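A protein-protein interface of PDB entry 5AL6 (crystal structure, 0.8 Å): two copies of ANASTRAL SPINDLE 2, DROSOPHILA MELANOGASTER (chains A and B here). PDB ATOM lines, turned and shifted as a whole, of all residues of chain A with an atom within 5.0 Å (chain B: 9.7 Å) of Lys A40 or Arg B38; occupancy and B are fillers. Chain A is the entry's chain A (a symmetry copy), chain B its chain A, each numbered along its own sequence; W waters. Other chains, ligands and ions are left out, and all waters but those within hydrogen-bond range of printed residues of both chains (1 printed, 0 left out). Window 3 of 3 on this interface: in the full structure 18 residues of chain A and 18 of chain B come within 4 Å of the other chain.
Water W1 lies within hydrogen-bond range of the guanidinium group of Arg B38 (3.0 Å) and the side-chain amino group of Lys A40 (3.2 Å).
Among the printed residues, pairs that only touch across the chains: Lys A40 with Gln B35, Lys A40 with Arg B38, Lys A40 with Ala B39 and Gly A43 with Phe B42.
Gln A36 touches its own counterpart, Gln B36. Lys A40 touches Arg B38, but with the chains exchanged Arg A38 does not touch Lys B40 (11.7 Å). Lys A40 touches Ala B39, but with the chains exchanged Ala A39 does not touch Lys B40 (9.2 Å). Gly A43 touches Phe B42, but with the chains exchanged Phe A42 does not touch Gly B43 (10.5 Å). Of the 8 pairs that touch across the chains among the printed residues, 1 has its exchanged pair printed and touching as well.
The side-chain amide nitrogen (NE2) of Gln A36 lies within hydrogen-bond range of the backbone carbonyl oxygen (O) of Ile B32 (3.2 Å). OE1 of Gln B35 sits at hydrogen-bond distance from NE2 of Gln A36 (2.6 Å). The side-chain amide nitrogen (NE2) of Gln B35 is in hydrogen-bond range of the side-chain amide oxygen (OE1) of Gln A37 (3.1 Å). OE1 of Gln A36 sits close to OE1 of Gln B36 (3.4 Å).
Arg B38 touches one residue of chain A. No residue of chain B comes within 4 Å of Ala A39. Of chain B, only Phe B42 (3.9 Å) comes within 4 Å of Gly A43. Of the printed residues of chain B, Gln A36 touches Ile B32, Gln B35 and Gln B36. Of the printed residues of chain A, Ala B39 touches Lys A40. Of the printed residues of chain A, Gln B35 touches Gln A36 (2.6 Å), Gln A37 (3.1 Å) and Lys A40 (3.7 Å). Printed residues of chain B within 4 Å of Gln A37: Gln B35. Of the printed residues of chain A, Ile B32 touches Gln A36. Glu B41 touches none of the printed residues of chain A. Glu A44 touches none of the printed residues of chain B.
Among the printed residues, 8 pairs touch across the chains.
NE2 of Gln A37 lies within hydrogen-bond range of OE2 of Glu A41 (3.0 Å). The side-chain amino group (NZ) of Lys A40 lies within salt-bridge range of the side-chain carboxylate (OE2) of Glu A44 (2.8 Å).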
ATOM      1  N   GLN A  36     -29.397  -5.478  25.394  1.00  0.00           N
ATOM      2  CA  GLN A  36     -29.630  -4.036  25.400  1.00  0.00           C
ATOM      3  C   GLN A  36     -30.116  -3.555  24.039  1.00  0.00           C
ATOM      4  O   GLN A  36     -30.913  -2.614  24.008  1.00  0.00           O
ATOM      5  CB  GLN A  36     -28.401  -3.288  25.804  1.00  0.00           C
ATOM      6  CG  GLN A  36     -28.341  -1.830  25.516  1.00  0.00           C
ATOM      7  CD  GLN A  36     -26.874  -1.363  25.887  1.00  0.00           C
ATOM      8  OE1 GLN A  36     -26.529  -1.026  27.071  1.00  0.00           O
ATOM      9  NE2 GLN A  36     -25.967  -1.514  24.888  1.00  0.00           N
ATOM     10  N   GLN A  37     -29.656  -4.160  22.957  1.00  0.00           N
ATOM     11  CA  GLN A  37     -30.137  -3.766  21.650  1.00  0.00           C
ATOM     12  C   GLN A  37     -31.645  -4.050  21.516  1.00  0.00           C
ATOM     13  O   GLN A  37     -32.400  -3.252  20.962  1.00  0.00           O
ATOM     14  CB  GLN A  37     -29.333  -4.469  20.570  1.00  0.00           C
ATOM     15  CG  GLN A  37     -29.719  -3.993  19.200  1.00  0.00           C
ATOM     16  CD  GLN A  37     -28.793  -4.375  18.218  1.00  0.00           C
ATOM     17  OE1 GLN A  37     -27.567  -4.274  18.419  1.00  0.00           O
ATOM     18  NE2 GLN A  37     -29.356  -4.782  17.078  1.00  0.00           N
ATOM     19  N   ARG A  38     -32.079  -5.232  22.005  1.00  0.00           N
ATOM     20  CA  ARG A  38     -33.506  -5.534  21.972  1.00  0.00           C
ATOM     21  C   ARG A  38     -34.296  -4.510  22.801  1.00  0.00           C
ATOM     22  O   ARG A  38     -35.379  -4.076  22.381  1.00  0.00           O
ATOM     23  CB  ARG A  38     -33.794  -6.945  22.486  1.00  0.00           C
ATOM     24  CG  ARG A  38     -33.304  -8.008  21.507  1.00  0.00           C
ATOM     25  CD  ARG A  38     -33.798  -9.402  21.855  1.00  0.00           C
ATOM     26  NE  ARG A  38     -33.410  -9.839  23.181  1.00  0.00           N
ATOM     27  CZ  ARG A  38     -32.306 -10.534  23.478  1.00  0.00           C
ATOM     28  NH1 ARG A  38     -31.421 -10.790  22.528  1.00  0.00           N
ATOM     29  NH2 ARG A  38     -32.075 -10.945  24.718  1.00  0.00           N
ATOM     30  N   ALA A  39     -33.799  -4.135  23.979  1.00  0.00           N
ATOM     31  CA  ALA A  39     -34.510  -3.152  24.802  1.00  0.00           C
ATOM     32  C   ALA A  39     -34.570  -1.793  24.073  1.00  0.00           C
ATOM     33  O   ALA A  39     -35.606  -1.096  24.100  1.00  0.00           O
ATOM     34  CB  ALA A  39     -33.832  -2.967  26.163  1.00  0.00           C
ATOM     35  N   LYS A  40     -33.462  -1.409  23.452  1.00  0.00           N
ATOM     36  CA  LYS A  40     -33.397  -0.137  22.742  1.00  0.00           C
ATOM     37  C   LYS A  40     -34.392  -0.143  21.564  1.00  0.00           C
ATOM     38  O   LYS A  40     -35.140   0.831  21.367  1.00  0.00           O
ATOM     39  CB  LYS A  40     -31.951   0.065  22.285  1.00  0.00           C
ATOM     40  CG  LYS A  40     -31.701   1.375  21.551  1.00  0.00           C
ATOM     41  CD  LYS A  40     -30.209   1.548  21.267  1.00  0.00           C
ATOM     42  CE  LYS A  40     -29.827   2.877  20.634  1.00  0.00           C
ATOM     43  NZ  LYS A  40     -30.336   2.998  19.260  1.00  0.00           N
ATOM     44  N   GLU A  41     -34.404  -1.220  20.792  1.00  0.00           N
ATOM     45  CA  GLU A  41     -35.317  -1.330  19.666  1.00  0.00           C
ATOM     46  C   GLU A  41     -36.782  -1.342  20.125  1.00  0.00           C
ATOM     47  O   GLU A  41     -37.642  -0.794  19.432  1.00  0.00           O
ATOM     48  CB  GLU A  41     -34.983  -2.568  18.831  1.00  0.00           C
ATOM     49  CG  GLU A  41     -33.747  -2.369  18.039  1.00  0.00           C
ATOM     50  CD  GLU A  41     -33.324  -3.579  17.210  1.00  0.00           C
ATOM     51  OE1 GLU A  41     -34.197  -4.458  16.915  1.00  0.00           O
ATOM     52  OE2 GLU A  41     -32.114  -3.702  16.875  1.00  0.00           O
ATOM     53  N   PHE A  42     -37.075  -1.965  21.253  1.00  0.00           N
ATOM     54  CA  PHE A  42     -38.436  -1.929  21.812  1.00  0.00           C
ATOM     55  C   PHE A  42     -38.883  -0.482  22.049  1.00  0.00           C
ATOM     56  O   PHE A  42     -39.972  -0.074  21.635  1.00  0.00           O
ATOM     57  CB  PHE A  42     -38.442  -2.744  23.110  1.00  0.00           C
ATOM     58  CG  PHE A  42     -39.745  -2.634  23.881  1.00  0.00           C
ATOM     59  CD1 PHE A  42     -40.914  -3.179  23.371  1.00  0.00           C
ATOM     60  CD2 PHE A  42     -39.795  -2.027  25.088  1.00  0.00           C
ATOM     61  CE1 PHE A  42     -42.085  -3.147  24.108  1.00  0.00           C
ATOM     62  CE2 PHE A  42     -40.965  -2.003  25.843  1.00  0.00           C
ATOM     63  CZ  PHE A  42     -42.082  -2.562  25.327  1.00  0.00           C
ATOM     64  N   GLY A  43     -38.037   0.305  22.734  1.00  0.00           N
ATOM     65  CA  GLY A  43     -38.405   1.692  22.994  1.00  0.00           C
ATOM     66  C   GLY A  43     -38.616   2.482  21.703  1.00  0.00           C
ATOM     67  O   GLY A  43     -39.531   3.307  21.591  1.00  0.00           O
ATOM     68  N   GLU A  44     -37.749   2.247  20.745  1.00  0.00           N
ATOM     69  CA  GLU A  44     -37.870   2.894  19.459  1.00  0.00           C
ATOM     70  C   GLU A  44     -39.161   2.463  18.717  1.00  0.00           C
ATOM     71  O   GLU A  44     -39.800   3.285  18.066  1.00  0.00           O
ATOM     72  CB  GLU A  44     -36.607   2.623  18.665  1.00  0.00           C
ATOM     73  CG  GLU A  44     -35.394   3.354  19.275  1.00  0.00           C
ATOM     74  CD  GLU A  44     -34.038   2.825  18.867  1.00  0.00           C
ATOM     75  OE1 GLU A  44     -33.942   1.719  18.315  1.00  0.00           O
ATOM     76  OE2 GLU A  44     -33.041   3.530  19.207  1.00  0.00           O
ATOM     77  N   GLU B  30     -16.760  -1.174  24.598  1.00  0.00           N
ATOM     78  CA  GLU B  30     -16.929   0.204  24.155  1.00  0.00           C
ATOM     79  C   GLU B  30     -18.240   0.349  23.338  1.00  0.00           C
ATOM     80  O   GLU B  30     -18.956   1.348  23.491  1.00  0.00           O
ATOM     81  CB  GLU B  30     -15.742   0.671  23.306  1.00  0.00           C
ATOM     82  CG  GLU B  30     -14.400   0.712  24.048  1.00  0.00           C
ATOM     83  CD  GLU B  30     -14.220   1.898  24.963  1.00  0.00           C
ATOM     84  OE1 GLU B  30     -15.105   2.764  25.062  1.00  0.00           O
ATOM     85  OE2 GLU B  30     -13.182   1.939  25.665  1.00  0.00           O
ATOM     86  N   MET B  31     -18.538  -0.632  22.493  1.00  0.00           N
ATOM     87  CA  MET B  31     -19.798  -0.613  21.752  1.00  0.00           C
ATOM     88  C   MET B  31     -20.999  -0.693  22.701  1.00  0.00           C
ATOM     89  O   MET B  31     -22.027  -0.031  22.462  1.00  0.00           O
ATOM     90  CB  MET B  31     -19.852  -1.759  20.716  1.00  0.00           C
ATOM     91  CG  MET B  31     -18.756  -1.698  19.661  1.00  0.00           C
ATOM     92  SD  MET B  31     -18.824  -0.225  18.628  1.00  0.00           S
ATOM     93  CE  MET B  31     -20.056  -0.756  17.441  1.00  0.00           C
ATOM     94  N   ILE B  32     -20.905  -1.504  23.755  1.00  0.00           N
ATOM     95  CA  ILE B  32     -21.982  -1.564  24.748  1.00  0.00           C
ATOM     96  C   ILE B  32     -22.212  -0.179  25.371  1.00  0.00           C
ATOM     97  O   ILE B  32     -23.355   0.280  25.478  1.00  0.00           O
ATOM     98  CB  ILE B  32     -21.668  -2.621  25.836  1.00  0.00           C
ATOM     99  CG1 ILE B  32     -21.738  -4.039  25.252  1.00  0.00           C
ATOM    100  CG2 ILE B  32     -22.610  -2.482  27.037  1.00  0.00           C
ATOM    101  CD1 ILE B  32     -21.187  -5.132  26.152  1.00  0.00           C
ATOM    102  N   LEU B  33     -21.128   0.475  25.797  1.00  0.00           N
ATOM    103  CA  LEU B  33     -21.259   1.795  26.416  1.00  0.00           C
ATOM    104  C   LEU B  33     -21.920   2.783  25.443  1.00  0.00           C
ATOM    105  O   LEU B  33     -22.822   3.542  25.819  1.00  0.00           O
ATOM    106  CB  LEU B  33     -19.891   2.309  26.856  1.00  0.00           C
ATOM    107  CG  LEU B  33     -19.908   3.670  27.557  1.00  0.00           C
ATOM    108  CD1 LEU B  33     -20.420   3.558  28.998  1.00  0.00           C
ATOM    109  CD2 LEU B  33     -18.503   4.301  27.571  1.00  0.00           C
ATOM    110  N   GLU B  34     -21.434   2.803  24.196  1.00  0.00           N
ATOM    111  CA  GLU B  34     -21.940   3.763  23.222  1.00  0.00           C
ATOM    112  C   GLU B  34     -23.420   3.541  22.913  1.00  0.00           C
ATOM    113  O   GLU B  34     -24.207   4.503  22.826  1.00  0.00           O
ATOM    114  CB  GLU B  34     -21.121   3.670  21.917  1.00  0.00           C
ATOM    115  CG  GLU B  34     -19.688   4.158  22.124  1.00  0.00           C
ATOM    116  CD  GLU B  34     -18.694   3.680  21.112  1.00  0.00           C
ATOM    117  OE1 GLU B  34     -19.074   2.945  20.159  1.00  0.00           O
ATOM    118  OE2 GLU B  34     -17.510   3.984  21.240  1.00  0.00           O
ATOM    119  N   GLN B  35     -23.806   2.276  22.726  1.00  0.00           N
ATOM    120  CA  GLN B  35     -25.200   1.969  22.436  1.00  0.00           C
ATOM    121  C   GLN B  35     -26.103   2.317  23.624  1.00  0.00           C
ATOM    122  O   GLN B  35     -27.187   2.889  23.433  1.00  0.00           O
ATOM    123  CB  GLN B  35     -25.338   0.498  22.024  1.00  0.00           C
ATOM    124  CG  GLN B  35     -26.817   0.059  21.779  1.00  0.00           C
ATOM    125  CD  GLN B  35     -26.922  -1.499  21.532  1.00  0.00           C
ATOM    126  OE1 GLN B  35     -26.650  -2.309  22.485  1.00  0.00           O
ATOM    127  NE2 GLN B  35     -27.239  -1.913  20.365  1.00  0.00           N
ATOM    128  N   GLN B  36     -25.682   1.977  24.838  1.00  0.00           N
ATOM    129  CA  GLN B  36     -26.540   2.327  25.968  1.00  0.00           C
ATOM    130  C   GLN B  36     -26.638   3.838  26.133  1.00  0.00           C
ATOM    131  O   GLN B  36     -27.701   4.309  26.545  1.00  0.00           O
ATOM    132  CB  GLN B  36     -26.056   1.700  27.234  1.00  0.00           C
ATOM    133  CG  GLN B  36     -26.576   2.230  28.523  1.00  0.00           C
ATOM    134  CD  GLN B  36     -25.758   1.501  29.667  1.00  0.00           C
ATOM    135  OE1 GLN B  36     -26.086   0.358  30.137  1.00  0.00           O
ATOM    136  NE2 GLN B  36     -24.583   2.101  29.988  1.00  0.00           N
ATOM    137  N   GLN B  37     -25.580   4.573  25.836  1.00  0.00           N
ATOM    138  CA  GLN B  37     -25.653   6.016  25.928  1.00  0.00           C
ATOM    139  C   GLN B  37     -26.678   6.574  24.924  1.00  0.00           C
ATOM    140  O   GLN B  37     -27.443   7.487  25.231  1.00  0.00           O
ATOM    141  CB  GLN B  37     -24.273   6.617  25.719  1.00  0.00           C
ATOM    142  CG  GLN B  37     -24.285   8.104  25.930  1.00  0.00           C
ATOM    143  CD  GLN B  37     -22.995   8.637  26.061  1.00  0.00           C
ATOM    144  OE1 GLN B  37     -22.135   8.073  26.766  1.00  0.00           O
ATOM    145  NE2 GLN B  37     -22.825   9.797  25.421  1.00  0.00           N
ATOM    146  N   ARG B  38     -26.662   6.033  23.686  1.00  0.00           N
ATOM    147  CA  ARG B  38     -27.653   6.468  22.707  1.00  0.00           C
ATOM    148  C   ARG B  38     -29.074   6.157  23.199  1.00  0.00           C
ATOM    149  O   ARG B  38     -29.983   6.982  23.027  1.00  0.00           O
ATOM    150  CB  ARG B  38     -27.423   5.813  21.345  1.00  0.00           C
ATOM    151  CG  ARG B  38     -26.167   6.353  20.668  1.00  0.00           C
ATOM    152  CD  ARG B  38     -26.048   5.920  19.216  1.00  0.00           C
ATOM    153  NE  ARG B  38     -26.036   4.482  19.041  1.00  0.00           N
ATOM    154  CZ  ARG B  38     -24.942   3.714  18.997  1.00  0.00           C
ATOM    155  NH1 ARG B  38     -23.754   4.256  19.216  1.00  0.00           N
ATOM    156  NH2 ARG B  38     -25.036   2.411  18.763  1.00  0.00           N
ATOM    157  N   ALA B  39     -29.296   4.977  23.778  1.00  0.00           N
ATOM    158  CA  ALA B  39     -30.633   4.638  24.275  1.00  0.00           C
ATOM    159  C   ALA B  39     -31.036   5.596  25.415  1.00  0.00           C
ATOM    160  O   ALA B  39     -32.198   6.043  25.497  1.00  0.00           O
ATOM    161  CB  ALA B  39     -30.691   3.194  24.782  1.00  0.00           C
ATOM    162  N   LYS B  40     -30.092   5.886  26.301  1.00  0.00           N
ATOM    163  CA  LYS B  40     -30.361   6.769  27.430  1.00  0.00           C
ATOM    164  C   LYS B  40     -30.709   8.181  26.919  1.00  0.00           C
ATOM    165  O   LYS B  40     -31.686   8.796  27.383  1.00  0.00           O
ATOM    166  CB  LYS B  40     -29.123   6.761  28.330  1.00  0.00           C
ATOM    167  CG  LYS B  40     -29.253   7.614  29.584  1.00  0.00           C
ATOM    168  CD  LYS B  40     -28.030   7.425  30.483  1.00  0.00           C
ATOM    169  CE  LYS B  40     -28.102   8.145  31.820  1.00  0.00           C
ATOM    170  NZ  LYS B  40     -28.046   9.607  31.662  1.00  0.00           N
ATOM    171  N   GLU B  41     -29.927   8.690  25.979  1.00  0.00           N
ATOM    172  CA  GLU B  41     -30.181  10.008  25.419  1.00  0.00           C
ATOM    173  C   GLU B  41     -31.523  10.056  24.673  1.00  0.00           C
ATOM    174  O   GLU B  41     -32.203  11.084  24.712  1.00  0.00           O
ATOM    175  CB  GLU B  41     -29.023  10.432  24.513  1.00  0.00           C
ATOM    176  CG  GLU B  41     -27.825  10.802  25.303  1.00  0.00           C
ATOM    177  CD  GLU B  41     -26.612  11.197  24.465  1.00  0.00           C
ATOM    178  OE1 GLU B  41     -26.791  11.583  23.265  1.00  0.00           O
ATOM    179  OE2 GLU B  41     -25.458  11.090  24.966  1.00  0.00           O
ATOM    180  N   PHE B  42     -31.895   8.986  23.994  1.00  0.00           N
ATOM    181  CA  PHE B  42     -33.213   8.918  23.342  1.00  0.00           C
ATOM    182  C   PHE B  42     -34.332   9.125  24.369  1.00  0.00           C
ATOM    183  O   PHE B  42     -35.237   9.941  24.172  1.00  0.00           O
ATOM    184  CB  PHE B  42     -33.331   7.561  22.641  1.00  0.00           C
ATOM    185  CG  PHE B  42     -34.718   7.291  22.085  1.00  0.00           C
ATOM    186  CD1 PHE B  42     -35.209   8.038  21.023  1.00  0.00           C
ATOM    187  CD2 PHE B  42     -35.496   6.308  22.591  1.00  0.00           C
ATOM    188  CE1 PHE B  42     -36.439   7.742  20.466  1.00  0.00           C
ATOM    189  CE2 PHE B  42     -36.730   5.995  22.026  1.00  0.00           C
ATOM    190  CZ  PHE B  42     -37.170   6.727  20.979  1.00  0.00           C
ATOM    191  N   GLY B  43     -34.279   8.369  25.478  1.00  0.00           N
ATOM    192  CA  GLY B  43     -35.316   8.518  26.494  1.00  0.00           C
ATOM    193  C   GLY B  43     -35.363   9.935  27.064  1.00  0.00           C
ATOM    194  O   GLY B  43     -36.436  10.496  27.316  1.00  0.00           O
ATOM    195  N   GLU B  44     -34.197  10.494  27.292  1.00  0.00           N
ATOM    196  CA  GLU B  44     -34.107  11.850  27.784  1.00  0.00           C
ATOM    197  C   GLU B  44     -34.660  12.872  26.759  1.00  0.00           C
ATOM    198  O   GLU B  44     -35.307  13.841  27.145  1.00  0.00           O
ATOM    199  CB  GLU B  44     -32.669  12.121  28.182  1.00  0.00           C
ATOM    200  CG  GLU B  44     -32.267  11.304  29.426  1.00  0.00           C
ATOM    201  CD  GLU B  44     -30.782  11.139  29.649  1.00  0.00           C
ATOM    202  OE1 GLU B  44     -29.983  11.403  28.738  1.00  0.00           O
ATOM    203  OE2 GLU B  44     -30.439  10.637  30.761  1.00  0.00           O
ATOM    204  N   ASN B  45     -34.404  12.649  25.476  1.00  0.00           N
ATOM    205  CA  ASN B  45     -34.944  13.526  24.436  1.00  0.00           C
ATOM    206  C   ASN B  45     -36.459  13.499  24.412  1.00  0.00           C
ATOM    207  O   ASN B  45     -37.086  14.530  24.112  1.00  0.00           O
ATOM    208  CB  ASN B  45     -34.460  13.071  23.035  1.00  0.00           C
ATOM    209  CG  ASN B  45     -33.022  13.462  22.771  1.00  0.00           C
ATOM    210  OD1 ASN B  45     -32.379  14.191  23.568  1.00  0.00           O
ATOM    211  ND2 ASN B  45     -32.435  12.834  21.752  1.00  0.00           N
ATOM    212  N   LEU B  46     -37.071  12.375  24.718  1.00  0.00           N
ATOM    213  CA  LEU B  46     -38.516  12.286  24.728  1.00  0.00           C
ATOM    214  C   LEU B  46     -39.142  13.041  25.914  1.00  0.00           C
ATOM    215  O   LEU B  46     -40.261  13.505  25.814  1.00  0.00           O
ATOM    216  CB  LEU B  46     -38.987  10.832  24.769  1.00  0.00           C
ATOM    217  CG  LEU B  46     -38.640  10.047  23.541  1.00  0.00           C
ATOM    218  CD1 LEU B  46     -39.307   8.677  23.559  1.00  0.00           C
ATOM    219  CD2 LEU B  46     -39.039  10.678  22.296  1.00  0.00           C
HETATM  220  O   HOH W   1     -27.788   1.352  18.274  1.00  0.00           O
